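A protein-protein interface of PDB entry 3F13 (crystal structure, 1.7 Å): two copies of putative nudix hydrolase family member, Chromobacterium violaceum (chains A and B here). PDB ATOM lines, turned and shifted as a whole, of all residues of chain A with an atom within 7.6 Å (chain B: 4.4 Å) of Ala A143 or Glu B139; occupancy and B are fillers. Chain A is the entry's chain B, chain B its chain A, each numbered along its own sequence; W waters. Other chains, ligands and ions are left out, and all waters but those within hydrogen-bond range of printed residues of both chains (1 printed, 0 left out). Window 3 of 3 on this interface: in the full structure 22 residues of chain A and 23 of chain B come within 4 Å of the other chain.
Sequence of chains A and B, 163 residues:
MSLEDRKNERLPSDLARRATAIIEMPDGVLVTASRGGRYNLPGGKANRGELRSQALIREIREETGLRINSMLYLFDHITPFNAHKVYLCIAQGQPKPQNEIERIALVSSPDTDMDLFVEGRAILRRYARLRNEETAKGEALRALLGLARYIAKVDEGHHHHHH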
ATOM      1  N   LEU A  72       3.338  33.091   4.551  1.00  0.00           N
ATOM      2  CA  LEU A  72       2.186  33.559   5.286  1.00  0.00           C
ATOM      3  C   LEU A  72       2.428  34.998   5.734  1.00  0.00           C
ATOM      4  O   LEU A  72       3.362  35.256   6.501  1.00  0.00           O
ATOM      5  CB  LEU A  72       1.939  32.662   6.511  1.00  0.00           C
ATOM      6  CG  LEU A  72       0.888  33.210   7.467  1.00  0.00           C
ATOM      7  CD1 LEU A  72      -0.488  33.206   6.740  1.00  0.00           C
ATOM      8  CD2 LEU A  72       0.850  32.369   8.730  1.00  0.00           C
ATOM      9  N   LEU A  88       6.209  34.773   7.009  1.00  0.00           N
ATOM     10  CA  LEU A  88       6.855  33.517   7.409  1.00  0.00           C
ATOM     11  C   LEU A  88       6.925  32.716   6.117  1.00  0.00           C
ATOM     12  O   LEU A  88       5.893  32.531   5.458  1.00  0.00           O
ATOM     13  CB  LEU A  88       5.971  32.757   8.396  1.00  0.00           C
ATOM     14  CG  LEU A  88       6.506  31.370   8.817  1.00  0.00           C
ATOM     15  CD1 LEU A  88       7.781  31.466   9.641  1.00  0.00           C
ATOM     16  CD2 LEU A  88       5.452  30.590   9.619  1.00  0.00           C
ATOM     17  N   ILE A  90       8.404  29.266   3.755  1.00  0.00           N
ATOM     18  CA  ILE A  90       8.971  27.945   3.587  1.00  0.00           C
ATOM     19  C   ILE A  90       9.636  27.851   2.203  1.00  0.00           C
ATOM     20  O   ILE A  90       9.061  28.249   1.165  1.00  0.00           O
ATOM     21  CB  ILE A  90       7.867  26.855   3.497  1.00  0.00           C
ATOM     22  CG1 ILE A  90       6.741  27.083   4.487  1.00  0.00           C
ATOM     23  CG2 ILE A  90       8.490  25.450   3.486  1.00  0.00           C
ATOM     24  CD1 ILE A  90       5.857  25.851   4.596  1.00  0.00           C
ATOM     25  N   LYS A 137      -4.552  33.510  12.942  1.00  0.00           N
ATOM     26  CA  LYS A 137      -3.220  33.717  12.377  1.00  0.00           C
ATOM     27  C   LYS A 137      -2.119  32.922  13.097  1.00  0.00           C
ATOM     28  O   LYS A 137      -1.294  32.274  12.460  1.00  0.00           O
ATOM     29  CB  LYS A 137      -2.879  35.195  12.303  1.00  0.00           C
ATOM     30  CG  LYS A 137      -1.479  35.486  11.823  1.00  0.00           C
ATOM     31  CD  LYS A 137      -1.342  36.956  11.573  1.00  0.00           C
ATOM     32  CE  LYS A 137      -1.805  37.328  10.184  1.00  0.00           C
ATOM     33  NZ  LYS A 137      -1.678  38.806  10.042  1.00  0.00           N
ATOM     34  N   GLY A 138      -2.113  32.982  14.419  1.00  0.00           N
ATOM     35  CA  GLY A 138      -1.184  32.190  15.226  1.00  0.00           C
ATOM     36  C   GLY A 138      -1.301  30.723  14.875  1.00  0.00           C
ATOM     37  O   GLY A 138      -0.273  30.049  14.749  1.00  0.00           O
ATOM     38  N   GLU A 139      -2.539  30.228  14.682  1.00  0.00           N
ATOM     39  CA  GLU A 139      -2.757  28.815  14.350  1.00  0.00           C
ATOM     40  C   GLU A 139      -2.182  28.453  12.983  1.00  0.00           C
ATOM     41  O   GLU A 139      -1.558  27.403  12.827  1.00  0.00           O
ATOM     42  CB  GLU A 139      -4.245  28.440  14.386  1.00  0.00           C
ATOM     43  CG  GLU A 139      -4.825  28.362  15.793  1.00  0.00           C
ATOM     44  CD  GLU A 139      -6.231  27.785  15.783  1.00  0.00           C
ATOM     45  OE1 GLU A 139      -6.344  26.533  15.718  1.00  0.00           O
ATOM     46  OE2 GLU A 139      -7.214  28.577  15.799  1.00  0.00           O
ATOM     47  N   ALA A 140      -2.446  29.312  11.995  1.00  0.00           N
ATOM     48  CA  ALA A 140      -1.840  29.186  10.662  1.00  0.00           C
ATOM     49  C   ALA A 140      -0.315  29.212  10.712  1.00  0.00           C
ATOM     50  O   ALA A 140       0.335  28.389  10.088  1.00  0.00           O
ATOM     51  CB  ALA A 140      -2.346  30.281   9.771  1.00  0.00           C
ATOM     52  N   LEU A 141       0.249  30.140  11.474  1.00  0.00           N
ATOM     53  CA  LEU A 141       1.688  30.228  11.635  1.00  0.00           C
ATOM     54  C   LEU A 141       2.217  28.899  12.195  1.00  0.00           C
ATOM     55  O   LEU A 141       3.148  28.297  11.631  1.00  0.00           O
ATOM     56  CB  LEU A 141       2.007  31.407  12.560  1.00  0.00           C
ATOM     57  CG  LEU A 141       3.425  31.911  12.747  1.00  0.00           C
ATOM     58  CD1 LEU A 141       3.333  33.194  13.616  1.00  0.00           C
ATOM     59  CD2 LEU A 141       4.264  30.838  13.438  1.00  0.00           C
ATOM     60  N   ARG A 142       1.608  28.418  13.275  1.00  0.00           N
ATOM     61  CA  ARG A 142       2.092  27.182  13.901  1.00  0.00           C
ATOM     62  C   ARG A 142       1.933  25.977  12.975  1.00  0.00           C
ATOM     63  O   ARG A 142       2.781  25.076  12.966  1.00  0.00           O
ATOM     64  CB  ARG A 142       1.428  26.927  15.251  1.00  0.00           C
ATOM     65  CG  ARG A 142       1.917  27.884  16.408  1.00  0.00           C
ATOM     66  CD  ARG A 142       1.339  27.434  17.749  1.00  0.00           C
ATOM     67  NE  ARG A 142      -0.094  27.670  17.803  1.00  0.00           N
ATOM     68  CZ  ARG A 142      -0.644  28.863  17.988  1.00  0.00           C
ATOM     69  NH1 ARG A 142       0.119  29.948  18.148  1.00  0.00           N
ATOM     70  NH2 ARG A 142      -1.955  28.975  17.986  1.00  0.00           N
ATOM     71  N   ALA A 143       0.872  25.958  12.176  1.00  0.00           N
ATOM     72  CA  ALA A 143       0.700  24.848  11.251  1.00  0.00           C
ATOM     73  C   ALA A 143       1.764  24.883  10.160  1.00  0.00           C
ATOM     74  O   ALA A 143       2.260  23.839   9.718  1.00  0.00           O
ATOM     75  CB  ALA A 143      -0.714  24.817  10.673  1.00  0.00           C
ATOM     76  N   LEU A 144       2.120  26.085   9.697  1.00  0.00           N
ATOM     77  CA  LEU A 144       3.162  26.192   8.677  1.00  0.00           C
ATOM     78  C   LEU A 144       4.504  25.736   9.248  1.00  0.00           C
ATOM     79  O   LEU A 144       5.256  25.050   8.578  1.00  0.00           O
ATOM     80  CB  LEU A 144       3.233  27.609   8.093  1.00  0.00           C
ATOM     81  CG  LEU A 144       2.095  27.851   7.113  1.00  0.00           C
ATOM     82  CD1 LEU A 144       2.037  29.332   6.688  1.00  0.00           C
ATOM     83  CD2 LEU A 144       2.334  26.934   5.886  1.00  0.00           C
ATOM     84  N   LEU A 145       4.796  26.131  10.481  1.00  0.00           N
ATOM     85  CA  LEU A 145       6.008  25.689  11.168  1.00  0.00           C
ATOM     86  C   LEU A 145       6.072  24.148  11.271  1.00  0.00           C
ATOM     87  O   LEU A 145       7.113  23.514  11.000  1.00  0.00           O
ATOM     88  CB  LEU A 145       6.109  26.382  12.521  1.00  0.00           C
ATOM     89  CG  LEU A 145       6.538  27.847  12.360  1.00  0.00           C
ATOM     90  CD1 LEU A 145       6.647  28.488  13.733  1.00  0.00           C
ATOM     91  CD2 LEU A 145       7.856  27.997  11.597  1.00  0.00           C
ATOM     92  N   GLY A 146       4.928  23.551  11.564  1.00  0.00           N
ATOM     93  CA  GLY A 146       4.785  22.099  11.603  1.00  0.00           C
ATOM     94  C   GLY A 146       5.076  21.438  10.266  1.00  0.00           C
ATOM     95  O   GLY A 146       5.740  20.427  10.217  1.00  0.00           O
ATOM     96  N   LEU A 147       4.552  22.012   9.180  1.00  0.00           N
ATOM     97  CA  LEU A 147       4.906  21.616   7.835  1.00  0.00           C
ATOM     98  C   LEU A 147       6.417  21.660   7.610  1.00  0.00           C
ATOM     99  O   LEU A 147       7.019  20.679   7.156  1.00  0.00           O
ATOM    100  CB  LEU A 147       4.135  22.495   6.815  1.00  0.00           C
ATOM    101  CG  LEU A 147       4.389  22.101   5.350  1.00  0.00           C
ATOM    102  CD1 LEU A 147       4.203  20.600   5.120  1.00  0.00           C
ATOM    103  CD2 LEU A 147       3.481  22.915   4.440  1.00  0.00           C
ATOM    104  N   ALA A 148       7.056  22.774   7.914  1.00  0.00           N
ATOM    105  CA  ALA A 148       8.491  22.865   7.694  1.00  0.00           C
ATOM    106  C   ALA A 148       9.223  21.762   8.474  1.00  0.00           C
ATOM    107  O   ALA A 148      10.125  21.105   7.946  1.00  0.00           O
ATOM    108  CB  ALA A 148       8.989  24.212   8.100  1.00  0.00           C
ATOM    109  N   ARG A 149       8.823  21.565   9.719  1.00  0.00           N
ATOM    110  CA  ARG A 149       9.412  20.512  10.550  1.00  0.00           C
ATOM    111  C   ARG A 149       9.255  19.130   9.972  1.00  0.00           C
ATOM    112  O   ARG A 149      10.204  18.332  10.003  1.00  0.00           O
ATOM    113  CB  ARG A 149       8.814  20.551  11.937  1.00  0.00           C
ATOM    114  CG  ARG A 149       9.512  21.548  12.811  1.00  0.00           C
ATOM    115  CD  ARG A 149       9.193  21.328  14.278  1.00  0.00           C
ATOM    116  NE  ARG A 149       7.832  21.756  14.573  1.00  0.00           N
ATOM    117  CZ  ARG A 149       7.503  22.998  14.914  1.00  0.00           C
ATOM    118  NH1 ARG A 149       8.435  23.956  15.022  1.00  0.00           N
ATOM    119  NH2 ARG A 149       6.245  23.274  15.158  1.00  0.00           N
ATOM    120  N   THR B 135      -2.285  14.836   7.395  1.00  0.00           N
ATOM    121  CA  THR B 135      -0.868  15.034   7.096  1.00  0.00           C
ATOM    122  C   THR B 135      -0.494  16.456   7.493  1.00  0.00           C
ATOM    123  O   THR B 135      -1.374  17.252   7.730  1.00  0.00           O
ATOM    124  CB  THR B 135      -0.575  14.902   5.590  1.00  0.00           C
ATOM    125  OG1 THR B 135      -1.366  15.880   4.883  1.00  0.00           O
ATOM    126  CG2 THR B 135      -0.919  13.448   5.062  1.00  0.00           C
ATOM    127  N   ALA B 136       0.795  16.751   7.601  1.00  0.00           N
ATOM    128  CA  ALA B 136       1.275  18.113   7.942  1.00  0.00           C
ATOM    129  C   ALA B 136       0.735  19.118   6.924  1.00  0.00           C
ATOM    130  O   ALA B 136       0.253  20.199   7.313  1.00  0.00           O
ATOM    131  CB  ALA B 136       2.796  18.170   7.970  1.00  0.00           C
ATOM    132  N   LYS B 137       0.749  18.725   5.651  1.00  0.00           N
ATOM    133  CA  LYS B 137       0.196  19.594   4.583  1.00  0.00           C
ATOM    134  C   LYS B 137      -1.323  19.829   4.714  1.00  0.00           C
ATOM    135  O   LYS B 137      -1.793  20.978   4.606  1.00  0.00           O
ATOM    136  CB  LYS B 137       0.575  19.100   3.185  1.00  0.00           C
ATOM    137  CG  LYS B 137      -0.045  19.967   2.125  1.00  0.00           C
ATOM    138  CD  LYS B 137       0.716  19.760   0.874  1.00  0.00           C
ATOM    139  CE  LYS B 137       2.022  20.468   1.033  1.00  0.00           C
ATOM    140  NZ  LYS B 137       2.654  20.513  -0.303  1.00  0.00           N
ATOM    141  N   GLY B 138      -2.085  18.769   5.012  1.00  0.00           N
ATOM    142  CA  GLY B 138      -3.549  18.900   5.199  1.00  0.00           C
ATOM    143  C   GLY B 138      -3.827  19.817   6.385  1.00  0.00           C
ATOM    144  O   GLY B 138      -4.764  20.617   6.353  1.00  0.00           O
ATOM    145  N   GLU B 139      -3.012  19.707   7.432  1.00  0.00           N
ATOM    146  CA  GLU B 139      -3.199  20.563   8.637  1.00  0.00           C
ATOM    147  C   GLU B 139      -2.907  22.037   8.299  1.00  0.00           C
ATOM    148  O   GLU B 139      -3.625  22.941   8.697  1.00  0.00           O
ATOM    149  CB  GLU B 139      -2.340  20.045   9.795  1.00  0.00           C
ATOM    150  CG  GLU B 139      -2.791  18.626  10.186  1.00  0.00           C
ATOM    151  CD  GLU B 139      -2.052  17.974  11.369  1.00  0.00           C
ATOM    152  OE1 GLU B 139      -2.714  17.205  12.082  1.00  0.00           O
ATOM    153  OE2 GLU B 139      -0.829  18.173  11.572  1.00  0.00           O
ATOM    154  N   ALA B 140      -1.816  22.263   7.577  1.00  0.00           N
ATOM    155  CA  ALA B 140      -1.496  23.612   7.103  1.00  0.00           C
ATOM    156  C   ALA B 140      -2.608  24.217   6.228  1.00  0.00           C
ATOM    157  O   ALA B 140      -2.967  25.377   6.357  1.00  0.00           O
ATOM    158  CB  ALA B 140      -0.201  23.558   6.307  1.00  0.00           C
ATOM    159  N   LEU B 141      -3.117  23.426   5.300  1.00  0.00           N
ATOM    160  CA  LEU B 141      -4.192  23.878   4.432  1.00  0.00           C
ATOM    161  C   LEU B 141      -5.420  24.230   5.312  1.00  0.00           C
ATOM    162  O   LEU B 141      -6.035  25.278   5.151  1.00  0.00           O
ATOM    163  CB  LEU B 141      -4.526  22.744   3.491  1.00  0.00           C
ATOM    164  CG  LEU B 141      -5.552  22.978   2.401  1.00  0.00           C
ATOM    165  CD1 LEU B 141      -5.670  21.706   1.579  1.00  0.00           C
ATOM    166  CD2 LEU B 141      -6.815  23.274   3.040  1.00  0.00           C
ATOM    167  N   ARG B 142      -5.788  23.342   6.224  1.00  0.00           N
ATOM    168  CA  ARG B 142      -6.983  23.624   7.033  1.00  0.00           C
ATOM    169  C   ARG B 142      -6.783  24.866   7.892  1.00  0.00           C
ATOM    170  O   ARG B 142      -7.710  25.645   8.092  1.00  0.00           O
ATOM    171  CB  ARG B 142      -7.385  22.409   7.873  1.00  0.00           C
ATOM    172  CG  ARG B 142      -7.934  21.241   7.012  1.00  0.00           C
ATOM    173  CD  ARG B 142      -8.523  20.141   7.941  1.00  0.00           C
ATOM    174  NE  ARG B 142      -7.486  19.434   8.678  1.00  0.00           N
ATOM    175  CZ  ARG B 142      -6.771  18.452   8.140  1.00  0.00           C
ATOM    176  NH1 ARG B 142      -7.033  18.087   6.885  1.00  0.00           N
ATOM    177  NH2 ARG B 142      -5.853  17.806   8.861  1.00  0.00           N
ATOM    178  N   ALA B 143      -5.579  25.045   8.417  1.00  0.00           N
ATOM    179  CA  ALA B 143      -5.285  26.238   9.219  1.00  0.00           C
ATOM    180  C   ALA B 143      -5.396  27.488   8.372  1.00  0.00           C
ATOM    181  O   ALA B 143      -5.908  28.555   8.804  1.00  0.00           O
ATOM    182  CB  ALA B 143      -3.910  26.138   9.824  1.00  0.00           C
HETATM  183  O   HOH W   1       1.071  21.352   9.626  1.00  0.00           O
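Ala A140 touches Ala B143, and with the chains exchanged Ala A143 touches Ala B140. Ala A143 touches Glu B139, but with the chains exchanged Glu A139 does not touch Ala B143 (4.02 Å). Ala B143 touches its own counterpart, Ala A143. 7 positions are printed for both chains. Of the 5 pairs that touch across the chains among the printed residues, 3 have their exchanged pair printed and touching as well.
Among the printed residues, pairs that only touch across the chains: Ala A140 with Ala B143, Ala A143 with Glu B139, Ala A143 with Ala B140, Ala A143 with Ala B143 and Leu A147 with Lys B137.
Of the printed residues of chain B, Ala A143 touches Glu B139 (3.99 Å), Ala B140 (3.8 Å) and Ala B143 (3.6 Å). Printed residues of chain A within 4 Å of Glu B139: Ala A143 (3.99 Å). No residue of chain A comes within 4 Å of Gly B138. Of the printed residues of chain A, Ala B143 touches Ala A140 and Ala A143. Of the printed residues of chain A, Lys B137 touches Leu A147. Arg A149 touches none of the printed residues of chain B. Arg A142 touches none of the printed residues of chain B.
Hydrophobic or aromatic side chains of chain B within 4 Å of the printed part of chain A: Ala B143. Of the 16 printed residues of chain A, 3 touch a printed residue of chain B. Printed residues of chain A that touch a printed residue of chain B: Ala A140, Ala A143 and Leu A147. Hydrophobic or aromatic side chains of chain A within 4 Å of the printed part of chain B: Ala A143 and Leu A147.
Water W1 lies within hydrogen-bond range of O of Ala B136 (2.7 Å) and O of Ala A143 (2.8 Å).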
